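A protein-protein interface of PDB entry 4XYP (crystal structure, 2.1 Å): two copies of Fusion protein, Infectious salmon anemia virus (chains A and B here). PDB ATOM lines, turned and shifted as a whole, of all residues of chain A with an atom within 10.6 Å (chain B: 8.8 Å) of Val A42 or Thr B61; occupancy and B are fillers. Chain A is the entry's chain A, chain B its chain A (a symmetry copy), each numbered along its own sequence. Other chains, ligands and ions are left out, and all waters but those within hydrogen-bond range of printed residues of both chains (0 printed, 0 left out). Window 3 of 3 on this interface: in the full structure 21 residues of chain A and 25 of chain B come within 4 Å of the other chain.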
ATOM      1  N   GLN A  34      10.241  -0.936  12.448  1.00  0.00           N
ATOM      2  CA  GLN A  34      11.579  -0.846  11.880  1.00  0.00           C
ATOM      3  C   GLN A  34      12.394   0.150  12.695  1.00  0.00           C
ATOM      4  O   GLN A  34      13.538  -0.126  13.068  1.00  0.00           O
ATOM      5  CB  GLN A  34      11.513  -0.432  10.421  1.00  0.00           C
ATOM      6  CG  GLN A  34      12.722  -0.743   9.636  1.00  0.00           C
ATOM      7  CD  GLN A  34      12.530  -0.318   8.212  1.00  0.00           C
ATOM      8  OE1 GLN A  34      11.946   0.736   7.943  1.00  0.00           O
ATOM      9  NE2 GLN A  34      12.976  -1.148   7.289  1.00  0.00           N
ATOM     10  N   ALA A  35      11.785   1.281  13.030  1.00  0.00           N
ATOM     11  CA  ALA A  35      12.479   2.300  13.815  1.00  0.00           C
ATOM     12  C   ALA A  35      12.784   1.815  15.242  1.00  0.00           C
ATOM     13  O   ALA A  35      13.851   2.110  15.802  1.00  0.00           O
ATOM     14  CB  ALA A  35      11.654   3.585  13.866  1.00  0.00           C
ATOM     15  N   SER A  36      11.847   1.090  15.856  1.00  0.00           N
ATOM     16  CA  SER A  36      12.075   0.544  17.202  1.00  0.00           C
ATOM     17  C   SER A  36      13.162  -0.515  17.232  1.00  0.00           C
ATOM     18  O   SER A  36      13.991  -0.574  18.171  1.00  0.00           O
ATOM     19  CB  SER A  36      10.804  -0.072  17.773  1.00  0.00           C
ATOM     20  OG  SER A  36       9.840   0.930  17.992  1.00  0.00           O
ATOM     21  N   SER A  37      13.162  -1.379  16.229  1.00  0.00           N
ATOM     22  CA  SER A  37      14.183  -2.423  16.201  1.00  0.00           C
ATOM     23  C   SER A  37      15.561  -1.807  15.899  1.00  0.00           C
ATOM     24  O   SER A  37      16.565  -2.268  16.427  1.00  0.00           O
ATOM     25  CB  SER A  37      13.803  -3.526  15.201  1.00  0.00           C
ATOM     26  OG  SER A  37      13.881  -3.034  13.877  1.00  0.00           O
ATOM     27  N   LEU A  38      15.648  -0.758  15.089  1.00  0.00           N
ATOM     28  CA  LEU A  38      16.934  -0.070  14.947  1.00  0.00           C
ATOM     29  C   LEU A  38      17.390   0.550  16.277  1.00  0.00           C
ATOM     30  O   LEU A  38      18.536   0.379  16.701  1.00  0.00           O
ATOM     31  CB  LEU A  38      16.847   1.010  13.872  1.00  0.00           C
ATOM     32  CG  LEU A  38      18.062   1.929  13.825  1.00  0.00           C
ATOM     33  CD1 LEU A  38      19.267   1.114  13.417  1.00  0.00           C
ATOM     34  CD2 LEU A  38      17.834   3.100  12.899  1.00  0.00           C
ATOM     35  N   GLN A  39      16.506   1.299  16.926  1.00  0.00           N
ATOM     36  CA  GLN A  39      16.802   1.849  18.235  1.00  0.00           C
ATOM     37  C   GLN A  39      17.278   0.826  19.242  1.00  0.00           C
ATOM     38  O   GLN A  39      18.251   1.071  19.972  1.00  0.00           O
ATOM     39  CB  GLN A  39      15.590   2.534  18.844  1.00  0.00           C
ATOM     40  CG  GLN A  39      15.930   3.264  20.092  1.00  0.00           C
ATOM     41  CD  GLN A  39      14.752   4.010  20.633  1.00  0.00           C
ATOM     42  OE1 GLN A  39      14.427   5.093  20.153  1.00  0.00           O
ATOM     43  NE2 GLN A  39      14.097   3.436  21.634  1.00  0.00           N
ATOM     44  N   ASN A  40      16.548  -0.282  19.349  1.00  0.00           N
ATOM     45  CA  ASN A  40      16.964  -1.364  20.247  1.00  0.00           C
ATOM     46  C   ASN A  40      18.327  -1.934  19.885  1.00  0.00           C
ATOM     47  O   ASN A  40      19.164  -2.191  20.772  1.00  0.00           O
ATOM     48  CB  ASN A  40      15.909  -2.478  20.272  1.00  0.00           C
ATOM     49  CG  ASN A  40      14.600  -2.022  20.920  1.00  0.00           C
ATOM     50  OD1 ASN A  40      14.591  -1.051  21.649  1.00  0.00           O
ATOM     51  ND2 ASN A  40      13.507  -2.723  20.649  1.00  0.00           N
ATOM     52  N   GLN A  41      18.596  -2.084  18.592  1.00  0.00           N
ATOM     53  CA  GLN A  41      19.900  -2.626  18.176  1.00  0.00           C
ATOM     54  C   GLN A  41      21.013  -1.670  18.585  1.00  0.00           C
ATOM     55  O   GLN A  41      22.068  -2.075  19.060  1.00  0.00           O
ATOM     56  CB  GLN A  41      19.922  -2.882  16.673  1.00  0.00           C
ATOM     57  CG  GLN A  41      21.255  -3.425  16.155  1.00  0.00           C
ATOM     58  CD  GLN A  41      21.151  -3.971  14.714  1.00  0.00           C
ATOM     59  OE1 GLN A  41      20.104  -3.882  14.073  1.00  0.00           O
ATOM     60  NE2 GLN A  41      22.238  -4.567  14.223  1.00  0.00           N
ATOM     61  N   VAL A  42      20.765  -0.379  18.442  1.00  0.00           N
ATOM     62  CA  VAL A  42      21.748   0.625  18.813  1.00  0.00           C
ATOM     63  C   VAL A  42      22.045   0.545  20.299  1.00  0.00           C
ATOM     64  O   VAL A  42      23.207   0.504  20.749  1.00  0.00           O
ATOM     65  CB  VAL A  42      21.224   2.021  18.446  1.00  0.00           C
ATOM     66  CG1 VAL A  42      21.965   3.111  19.169  1.00  0.00           C
ATOM     67  CG2 VAL A  42      21.323   2.222  16.976  1.00  0.00           C
ATOM     68  N   GLU A  43      20.976   0.523  21.077  1.00  0.00           N
ATOM     69  CA  GLU A  43      21.120   0.536  22.531  1.00  0.00           C
ATOM     70  C   GLU A  43      21.797  -0.713  23.086  1.00  0.00           C
ATOM     71  O   GLU A  43      22.684  -0.655  23.949  1.00  0.00           O
ATOM     72  CB  GLU A  43      19.761   0.714  23.162  1.00  0.00           C
ATOM     73  CG  GLU A  43      19.820   1.142  24.601  1.00  0.00           C
ATOM     74  CD  GLU A  43      18.424   1.479  25.141  1.00  0.00           C
ATOM     75  OE1 GLU A  43      17.464   1.564  24.332  1.00  0.00           O
ATOM     76  OE2 GLU A  43      18.284   1.637  26.374  1.00  0.00           O
ATOM     77  N   ILE A  44      21.378  -1.855  22.591  1.00  0.00           N
ATOM     78  CA  ILE A  44      22.064  -3.107  22.892  1.00  0.00           C
ATOM     79  C   ILE A  44      23.546  -3.010  22.519  1.00  0.00           C
ATOM     80  O   ILE A  44      24.437  -3.405  23.291  1.00  0.00           O
ATOM     81  CB  ILE A  44      21.412  -4.265  22.130  1.00  0.00           C
ATOM     82  CG1 ILE A  44      20.005  -4.488  22.652  1.00  0.00           C
ATOM     83  CG2 ILE A  44      22.241  -5.517  22.257  1.00  0.00           C
ATOM     84  CD1 ILE A  44      19.199  -5.339  21.680  1.00  0.00           C
ATOM     85  N   GLY A  45      23.807  -2.473  21.338  1.00  0.00           N
ATOM     86  CA  GLY A  45      25.178  -2.276  20.886  1.00  0.00           C
ATOM     87  C   GLY A  45      26.009  -1.401  21.810  1.00  0.00           C
ATOM     88  O   GLY A  45      27.204  -1.648  22.030  1.00  0.00           O
ATOM     89  N   LEU A  46      25.385  -0.360  22.349  1.00  0.00           N
ATOM     90  CA  LEU A  46      26.073   0.539  23.266  1.00  0.00           C
ATOM     91  C   LEU A  46      26.353  -0.171  24.586  1.00  0.00           C
ATOM     92  O   LEU A  46      27.423  -0.026  25.219  1.00  0.00           O
ATOM     93  CB  LEU A  46      25.223   1.803  23.528  1.00  0.00           C
ATOM     94  CG  LEU A  46      25.034   2.717  22.314  1.00  0.00           C
ATOM     95  CD1 LEU A  46      24.096   3.849  22.612  1.00  0.00           C
ATOM     96  CD2 LEU A  46      26.358   3.260  21.837  1.00  0.00           C
ATOM     97  N   ILE A  47      25.382  -0.932  25.056  1.00  0.00           N
ATOM     98  CA  ILE A  47      25.619  -1.628  26.300  1.00  0.00           C
ATOM     99  C   ILE A  47      26.788  -2.593  26.119  1.00  0.00           C
ATOM    100  O   ILE A  47      27.683  -2.727  26.984  1.00  0.00           O
ATOM    101  CB  ILE A  47      24.369  -2.375  26.775  1.00  0.00           C
ATOM    102  CG1 ILE A  47      23.339  -1.351  27.259  1.00  0.00           C
ATOM    103  CG2 ILE A  47      24.744  -3.350  27.863  1.00  0.00           C
ATOM    104  CD1 ILE A  47      21.976  -1.891  27.573  1.00  0.00           C
ATOM    105  N   GLY A  48      26.784  -3.290  25.006  1.00  0.00           N
ATOM    106  CA  GLY A  48      27.892  -4.192  24.700  1.00  0.00           C
ATOM    107  C   GLY A  48      29.235  -3.494  24.768  1.00  0.00           C
ATOM    108  O   GLY A  48      30.191  -4.017  25.346  1.00  0.00           O
ATOM    109  N   GLU A  49      29.313  -2.297  24.198  1.00  0.00           N
ATOM    110  CA  GLU A  49      30.566  -1.551  24.211  1.00  0.00           C
ATOM    111  C   GLU A  49      30.932  -1.095  25.602  1.00  0.00           C
ATOM    112  O   GLU A  49      32.102  -1.036  25.964  1.00  0.00           O
ATOM    113  CB  GLU A  49      30.467  -0.322  23.327  1.00  0.00           C
ATOM    114  CG  GLU A  49      30.143  -0.621  21.885  1.00  0.00           C
ATOM    115  CD  GLU A  49      29.552   0.584  21.175  1.00  0.00           C
ATOM    116  OE1 GLU A  49      30.074   1.701  21.412  1.00  0.00           O
ATOM    117  OE2 GLU A  49      28.570   0.421  20.399  1.00  0.00           O
ATOM    118  N   TYR A  50      29.918  -0.714  26.372  1.00  0.00           N
ATOM    119  CA  TYR A  50      30.151  -0.261  27.727  1.00  0.00           C
ATOM    120  C   TYR A  50      30.783  -1.368  28.552  1.00  0.00           C
ATOM    121  O   TYR A  50      31.721  -1.140  29.310  1.00  0.00           O
ATOM    122  CB  TYR A  50      28.856   0.180  28.363  1.00  0.00           C
ATOM    123  CG  TYR A  50      29.009   0.606  29.807  1.00  0.00           C
ATOM    124  CD1 TYR A  50      29.604   1.819  30.145  1.00  0.00           C
ATOM    125  CD2 TYR A  50      28.554  -0.203  30.816  1.00  0.00           C
ATOM    126  CE1 TYR A  50      29.739   2.197  31.454  1.00  0.00           C
ATOM    127  CE2 TYR A  50      28.685   0.159  32.132  1.00  0.00           C
ATOM    128  CZ  TYR A  50      29.284   1.358  32.445  1.00  0.00           C
ATOM    129  OH  TYR A  50      29.413   1.702  33.758  1.00  0.00           O
ATOM    130  N   SER A  54      31.873  -6.430  23.153  1.00  0.00           N
ATOM    131  CA  SER A  54      31.213  -6.290  21.862  1.00  0.00           C
ATOM    132  C   SER A  54      31.499  -7.446  20.898  1.00  0.00           C
ATOM    133  O   SER A  54      30.581  -8.023  20.339  1.00  0.00           O
ATOM    134  CB  SER A  54      31.635  -4.964  21.177  1.00  0.00           C
ATOM    135  OG  SER A  54      31.523  -3.859  22.041  1.00  0.00           O
ATOM    136  N   LEU A  57      30.155 -10.988  22.056  1.00  0.00           N
ATOM    137  CA  LEU A  57      28.700 -10.925  22.158  1.00  0.00           C
ATOM    138  C   LEU A  57      28.062 -11.008  20.772  1.00  0.00           C
ATOM    139  O   LEU A  57      27.088 -11.718  20.563  1.00  0.00           O
ATOM    140  CB  LEU A  57      28.320  -9.628  22.858  1.00  0.00           C
ATOM    141  CG  LEU A  57      26.854  -9.252  22.904  1.00  0.00           C
ATOM    142  CD1 LEU A  57      26.026 -10.271  23.626  1.00  0.00           C
ATOM    143  CD2 LEU A  57      26.770  -7.855  23.547  1.00  0.00           C
ATOM    144  N   GLU A  58      28.670 -10.298  19.823  1.00  0.00           N
ATOM    145  CA  GLU A  58      28.248 -10.274  18.432  1.00  0.00           C
ATOM    146  C   GLU A  58      28.324 -11.654  17.766  1.00  0.00           C
ATOM    147  O   GLU A  58      27.435 -12.039  17.027  1.00  0.00           O
ATOM    148  CB  GLU A  58      29.147  -9.309  17.658  1.00  0.00           C
ATOM    149  CG  GLU A  58      28.507  -8.212  16.861  1.00  0.00           C
ATOM    150  CD  GLU A  58      29.580  -7.344  16.193  1.00  0.00           C
ATOM    151  OE1 GLU A  58      30.114  -6.413  16.845  1.00  0.00           O
ATOM    152  OE2 GLU A  58      29.923  -7.630  15.027  1.00  0.00           O
ATOM    153  N   GLN B  41      12.645  -3.450  24.232  1.00  0.00           N
ATOM    154  CA  GLN B  41      12.933  -2.100  24.743  1.00  0.00           C
ATOM    155  C   GLN B  41      12.883  -2.100  26.266  1.00  0.00           C
ATOM    156  O   GLN B  41      13.712  -1.496  26.938  1.00  0.00           O
ATOM    157  CB  GLN B  41      11.954  -1.084  24.163  1.00  0.00           C
ATOM    158  CG  GLN B  41      12.171   0.345  24.666  1.00  0.00           C
ATOM    159  CD  GLN B  41      11.394   1.388  23.834  1.00  0.00           C
ATOM    160  OE1 GLN B  41      10.635   1.043  22.927  1.00  0.00           O
ATOM    161  NE2 GLN B  41      11.613   2.669  24.131  1.00  0.00           N
ATOM    162  N   ILE B  44      16.114  -4.100  27.597  1.00  0.00           N
ATOM    163  CA  ILE B  44      17.258  -3.209  27.431  1.00  0.00           C
ATOM    164  C   ILE B  44      17.221  -2.089  28.474  1.00  0.00           C
ATOM    165  O   ILE B  44      18.235  -1.768  29.118  1.00  0.00           O
ATOM    166  CB  ILE B  44      17.258  -2.607  26.023  1.00  0.00           C
ATOM    167  CG1 ILE B  44      17.502  -3.703  25.001  1.00  0.00           C
ATOM    168  CG2 ILE B  44      18.300  -1.522  25.910  1.00  0.00           C
ATOM    169  CD1 ILE B  44      17.122  -3.230  23.604  1.00  0.00           C
ATOM    170  N   ILE B  53      23.371   3.330  34.087  1.00  0.00           N
ATOM    171  CA  ILE B  53      23.888   4.174  33.008  1.00  0.00           C
ATOM    172  C   ILE B  53      22.756   4.703  32.194  1.00  0.00           C
ATOM    173  O   ILE B  53      22.974   5.199  31.109  1.00  0.00           O
ATOM    174  CB  ILE B  53      24.888   3.371  32.086  1.00  0.00           C
ATOM    175  CG1 ILE B  53      24.248   2.074  31.586  1.00  0.00           C
ATOM    176  CG2 ILE B  53      26.135   3.015  32.841  1.00  0.00           C
ATOM    177  CD1 ILE B  53      24.981   1.354  30.460  1.00  0.00           C
ATOM    178  N   SER B  54      21.533   4.601  32.726  1.00  0.00           N
ATOM    179  CA  SER B  54      20.330   4.857  31.945  1.00  0.00           C
ATOM    180  C   SER B  54      20.371   6.179  31.171  1.00  0.00           C
ATOM    181  O   SER B  54      20.114   6.203  29.979  1.00  0.00           O
ATOM    182  CB  SER B  54      19.079   4.863  32.862  1.00  0.00           C
ATOM    183  OG  SER B  54      19.030   3.737  33.705  1.00  0.00           O
ATOM    184  N   SER B  55      20.676   7.287  31.840  1.00  0.00           N
ATOM    185  CA  SER B  55      20.523   8.595  31.190  1.00  0.00           C
ATOM    186  C   SER B  55      21.502   8.792  30.024  1.00  0.00           C
ATOM    187  O   SER B  55      21.128   9.248  28.955  1.00  0.00           O
ATOM    188  CB  SER B  55      20.704   9.718  32.203  1.00  0.00           C
ATOM    189  OG  SER B  55      19.705   9.640  33.198  1.00  0.00           O
ATOM    190  N   TRP B  56      22.758   8.423  30.222  1.00  0.00           N
ATOM    191  CA  TRP B  56      23.738   8.636  29.166  1.00  0.00           C
ATOM    192  C   TRP B  56      23.547   7.638  28.026  1.00  0.00           C
ATOM    193  O   TRP B  56      23.731   7.978  26.858  1.00  0.00           O
ATOM    194  CB  TRP B  56      25.159   8.547  29.710  1.00  0.00           C
ATOM    195  CG  TRP B  56      26.132   8.958  28.685  1.00  0.00           C
ATOM    196  CD1 TRP B  56      27.041   8.167  28.030  1.00  0.00           C
ATOM    197  CD2 TRP B  56      26.275  10.273  28.145  1.00  0.00           C
ATOM    198  NE1 TRP B  56      27.744   8.925  27.121  1.00  0.00           N
ATOM    199  CE2 TRP B  56      27.293  10.218  27.178  1.00  0.00           C
ATOM    200  CE3 TRP B  56      25.643  11.491  28.393  1.00  0.00           C
ATOM    201  CZ2 TRP B  56      27.698  11.342  26.470  1.00  0.00           C
ATOM    202  CZ3 TRP B  56      26.048  12.601  27.690  1.00  0.00           C
ATOM    203  CH2 TRP B  56      27.064  12.520  26.745  1.00  0.00           C
ATOM    204  N   LEU B  57      23.159   6.412  28.367  1.00  0.00           N
ATOM    205  CA  LEU B  57      22.896   5.388  27.361  1.00  0.00           C
ATOM    206  C   LEU B  57      21.763   5.824  26.433  1.00  0.00           C
ATOM    207  O   LEU B  57      21.842   5.675  25.222  1.00  0.00           O
ATOM    208  CB  LEU B  57      22.549   4.088  28.074  1.00  0.00           C
ATOM    209  CG  LEU B  57      22.049   2.931  27.234  1.00  0.00           C
ATOM    210  CD1 LEU B  57      23.055   2.489  26.215  1.00  0.00           C
ATOM    211  CD2 LEU B  57      21.658   1.806  28.210  1.00  0.00           C
ATOM    212  N   GLU B  58      20.731   6.412  27.035  1.00  0.00           N
ATOM    213  CA  GLU B  58      19.572   6.937  26.330  1.00  0.00           C
ATOM    214  C   GLU B  58      19.934   8.062  25.352  1.00  0.00           C
ATOM    215  O   GLU B  58      19.427   8.113  24.246  1.00  0.00           O
ATOM    216  CB  GLU B  58      18.575   7.482  27.353  1.00  0.00           C
ATOM    217  CG  GLU B  58      17.161   6.985  27.314  1.00  0.00           C
ATOM    218  CD  GLU B  58      16.338   7.629  28.439  1.00  0.00           C
ATOM    219  OE1 GLU B  58      16.370   7.127  29.589  1.00  0.00           O
ATOM    220  OE2 GLU B  58      15.700   8.670  28.176  1.00  0.00           O
ATOM    221  N   THR B  59      20.769   9.004  25.779  1.00  0.00           N
ATOM    222  CA  THR B  59      21.045  10.129  24.890  1.00  0.00           C
ATOM    223  C   THR B  59      21.893   9.597  23.735  1.00  0.00           C
ATOM    224  O   THR B  59      21.602   9.828  22.567  1.00  0.00           O
ATOM    225  CB  THR B  59      21.726  11.301  25.621  1.00  0.00           C
ATOM    226  OG1 THR B  59      21.971  12.365  24.681  1.00  0.00           O
ATOM    227  CG2 THR B  59      22.978  10.888  26.268  1.00  0.00           C
ATOM    228  N   LYS B  60      22.874   8.789  24.052  1.00  0.00           N
ATOM    229  CA  LYS B  60      23.670   8.198  23.003  1.00  0.00           C
ATOM    230  C   LYS B  60      22.772   7.402  22.088  1.00  0.00           C
ATOM    231  O   LYS B  60      22.924   7.485  20.868  1.00  0.00           O
ATOM    232  CB  LYS B  60      24.779   7.342  23.588  1.00  0.00           C
ATOM    233  CG  LYS B  60      26.053   8.115  23.958  1.00  0.00           C
ATOM    234  CD  LYS B  60      26.681   8.794  22.716  1.00  0.00           C
ATOM    235  CE  LYS B  60      28.202   8.592  22.621  1.00  0.00           C
ATOM    236  NZ  LYS B  60      28.709   8.882  21.239  1.00  0.00           N
ATOM    237  N   THR B  61      21.768   6.715  22.658  1.00  0.00           N
ATOM    238  CA  THR B  61      20.901   5.855  21.854  1.00  0.00           C
ATOM    239  C   THR B  61      20.017   6.630  20.890  1.00  0.00           C
ATOM    240  O   THR B  61      19.835   6.246  19.729  1.00  0.00           O
ATOM    241  CB  THR B  61      19.970   5.002  22.726  1.00  0.00           C
ATOM    242  OG1 THR B  61      20.709   3.955  23.371  1.00  0.00           O
ATOM    243  CG2 THR B  61      18.911   4.343  21.864  1.00  0.00           C
ATOM    244  N   LEU B  62      19.392   7.681  21.401  1.00  0.00           N
ATOM    245  CA  LEU B  62      18.468   8.470  20.603  1.00  0.00           C
ATOM    246  C   LEU B  62      19.183   9.173  19.447  1.00  0.00           C
ATOM    247  O   LEU B  62      18.659   9.237  18.335  1.00  0.00           O
ATOM    248  CB  LEU B  62      17.763   9.507  21.475  1.00  0.00           C
ATOM    249  CG  LEU B  62      16.925   8.879  22.577  1.00  0.00           C
ATOM    250  CD1 LEU B  62      16.507   9.916  23.634  1.00  0.00           C
ATOM    251  CD2 LEU B  62      15.742   8.186  21.922  1.00  0.00           C
ATOM    252  N   THR B  63      20.391   9.674  19.696  1.00  0.00           N
ATOM    253  CA  THR B  63      21.082  10.418  18.639  1.00  0.00           C
ATOM    254  C   THR B  63      21.643   9.490  17.574  1.00  0.00           C
ATOM    255  O   THR B  63      21.549   9.784  16.379  1.00  0.00           O
ATOM    256  CB  THR B  63      22.190  11.310  19.193  1.00  0.00           C
ATOM    257  OG1 THR B  63      23.078  10.570  20.021  1.00  0.00           O
ATOM    258  CG2 THR B  63      21.582  12.414  20.025  1.00  0.00           C
ATOM    259  N   LYS B  64      22.206   8.359  17.979  1.00  0.00           N
ATOM    260  CA  LYS B  64      22.688   7.396  16.984  1.00  0.00           C
ATOM    261  C   LYS B  64      21.543   6.829  16.181  1.00  0.00           C
ATOM    262  O   LYS B  64      21.689   6.621  14.976  1.00  0.00           O
ATOM    263  CB  LYS B  64      23.470   6.272  17.649  1.00  0.00           C
ATOM    264  CG  LYS B  64      24.833   6.699  18.069  1.00  0.00           C
ATOM    265  CD  LYS B  64      25.604   5.551  18.718  1.00  0.00           C
ATOM    266  CE  LYS B  64      26.878   6.030  19.424  1.00  0.00           C
ATOM    267  NZ  LYS B  64      27.921   6.590  18.514  1.00  0.00           N
ATOM    268  N   THR B  65      20.401   6.591  16.836  1.00  0.00           N
ATOM    269  CA  THR B  65      19.236   6.065  16.135  1.00  0.00           C
ATOM    270  C   THR B  65      18.724   7.122  15.167  1.00  0.00           C
ATOM    271  O   THR B  65      18.442   6.832  14.000  1.00  0.00           O
ATOM    272  CB  THR B  65      18.099   5.627  17.111  1.00  0.00           C
ATOM    273  OG1 THR B  65      18.623   4.702  18.085  1.00  0.00           O
ATOM    274  CG2 THR B  65      16.958   4.959  16.339  1.00  0.00           C
ATOM    275  N   GLU B  66      18.602   8.362  15.626  1.00  0.00           N
ATOM    276  CA  GLU B  66      18.131   9.402  14.701  1.00  0.00           C
ATOM    277  C   GLU B  66      19.116   9.531  13.523  1.00  0.00           C
ATOM    278  O   GLU B  66      18.705   9.700  12.376  1.00  0.00           O
ATOM    279  CB  GLU B  66      17.923  10.731  15.425  1.00  0.00           C
ATOM    280  CG  GLU B  66      16.650  10.732  16.303  1.00  0.00           C
ATOM    281  CD  GLU B  66      16.671  11.739  17.459  1.00  0.00           C
ATOM    282  OE1 GLU B  66      17.757  12.159  17.923  1.00  0.00           O
ATOM    283  OE2 GLU B  66      15.573  12.101  17.919  1.00  0.00           O
ATOM    284  N   GLU B  67      20.407   9.379  13.788  1.00  0.00           N
ATOM    285  CA  GLU B  67      21.395   9.415  12.720  1.00  0.00           C
ATOM    286  C   GLU B  67      21.204   8.257  11.752  1.00  0.00           C
ATOM    287  O   GLU B  67      21.236   8.454  10.546  1.00  0.00           O
ATOM    288  CB  GLU B  67      22.806   9.383  13.292  1.00  0.00           C
ATOM    289  CG  GLU B  67      23.370  10.761  13.597  1.00  0.00           C
ATOM    290  CD  GLU B  67      24.624  10.687  14.434  1.00  0.00           C
ATOM    291  OE1 GLU B  67      25.006   9.557  14.784  1.00  0.00           O
ATOM    292  OE2 GLU B  67      25.222  11.743  14.746  1.00  0.00           O
ATOM    293  N   GLY B  68      20.991   7.056  12.279  1.00  0.00           N
ATOM    294  CA  GLY B  68      20.750   5.883  11.452  1.00  0.00           C
ATOM    295  C   GLY B  68      19.518   6.028  10.577  1.00  0.00           C
ATOM    296  O   GLY B  68      19.484   5.526   9.453  1.00  0.00           O
ATOM    297  N   LEU B  69      18.503   6.712  11.101  1.00  0.00           N
ATOM    298  CA  LEU B  69      17.272   6.962  10.360  1.00  0.00           C
ATOM    299  C   LEU B  69      17.433   8.171   9.409  1.00  0.00           C
ATOM    300  O   LEU B  69      16.564   8.429   8.580  1.00  0.00           O
ATOM    301  CB  LEU B  69      16.109   7.195  11.338  1.00  0.00           C
ATOM    302  CG  LEU B  69      15.774   6.040  12.300  1.00  0.00           C
ATOM    303  CD1 LEU B  69      14.759   6.440  13.384  1.00  0.00           C
ATOM    304  CD2 LEU B  69      15.265   4.845  11.524  1.00  0.00           C
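O of Ser A36 sits close to ND2 of Asn A40 (3.3 Å).
OG1 of Thr B61 sits at hydrogen-bond distance from O of Leu B57, 2.8 Å away.
O of Lys B60 lies within hydrogen-bond range of OG1 of Thr B63, 3.2 Å away.
O of Thr B61 sits at hydrogen-bond distance from OG1 of Thr B65, 2.6 Å away.
Among the printed residues, pairs that only touch across the chains: Glu A43 with Ile B44, Glu A43 with Thr B61, Ile A44 with Ile B44, Gln A39 with Thr B65, Leu A38 with Leu B69, Leu A46 with Thr B61, Leu A46 with Leu B57, Tyr A50 with Ile B53, Gln A39 with Gln B41, Asn A40 with Ile B44, Gln A39 with Thr B61, Asn A40 with Gln B41, Leu A46 with Lys B60, Ile A47 with Leu B57, Leu A46 with Lys B64, Val A42 with Thr B65, Gln A39 with Leu B62, Val A42 with Lys B64, Val A42 with Thr B61, Glu A43 with Leu B57 and Leu A38 with Thr B65.
Of chain B, only Ile B44 (3.1 Å), Leu B57 (3.8 Å) and Thr B61 (3.2 Å) come within 4 Å of Glu A43.
No residue of chain B comes within 4 Å of Gly A45.
Of the printed residues of chain B, Tyr A50 touches Ile B53 (3.6 Å).
Leu B57 touches just these residues of chain A: Glu A43, Leu A46 and Ile A47.
No residue of chain A comes within 4 Å of Thr B59.
Thr B61 touches just these residues of chain A: Gln A39 (3.6 Å), Val A42 (3.8 Å), Glu A43 (3.2 Å) and Leu A46 (3.5 Å).
No residue of chain A comes within 4 Å of Thr B63.
Thr B65 touches just these residues of chain A: Leu A38, Gln A39 and Val A42.
Of the printed residues of chain A, Leu B69 touches Leu A38 (3.4 Å).
The nearest residue of chain B that does not touch Val A42 is Lys B60 (4.8 Å).
The nearest residue of chain A that does not touch Thr B61 is Asn A40 (5.8 Å).
The nearest printed residue of chain B that does not touch Ile A47 is Ile B44 (4.05 Å).
Hydrophobic or aromatic side chains of chain B that line the printed part of chain A: Ile B44, Ile B53, Leu B57, Leu B62 and Leu B69.
Of the 20 printed residues of chain A, 9 touch a printed residue of chain B.
Among the printed residues, no Asp or Glu carboxylate lies within 4 Å of a Lys or Arg side-chain nitrogen of the other chain.
Ile B44 touches its own counterpart, Ile A44.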
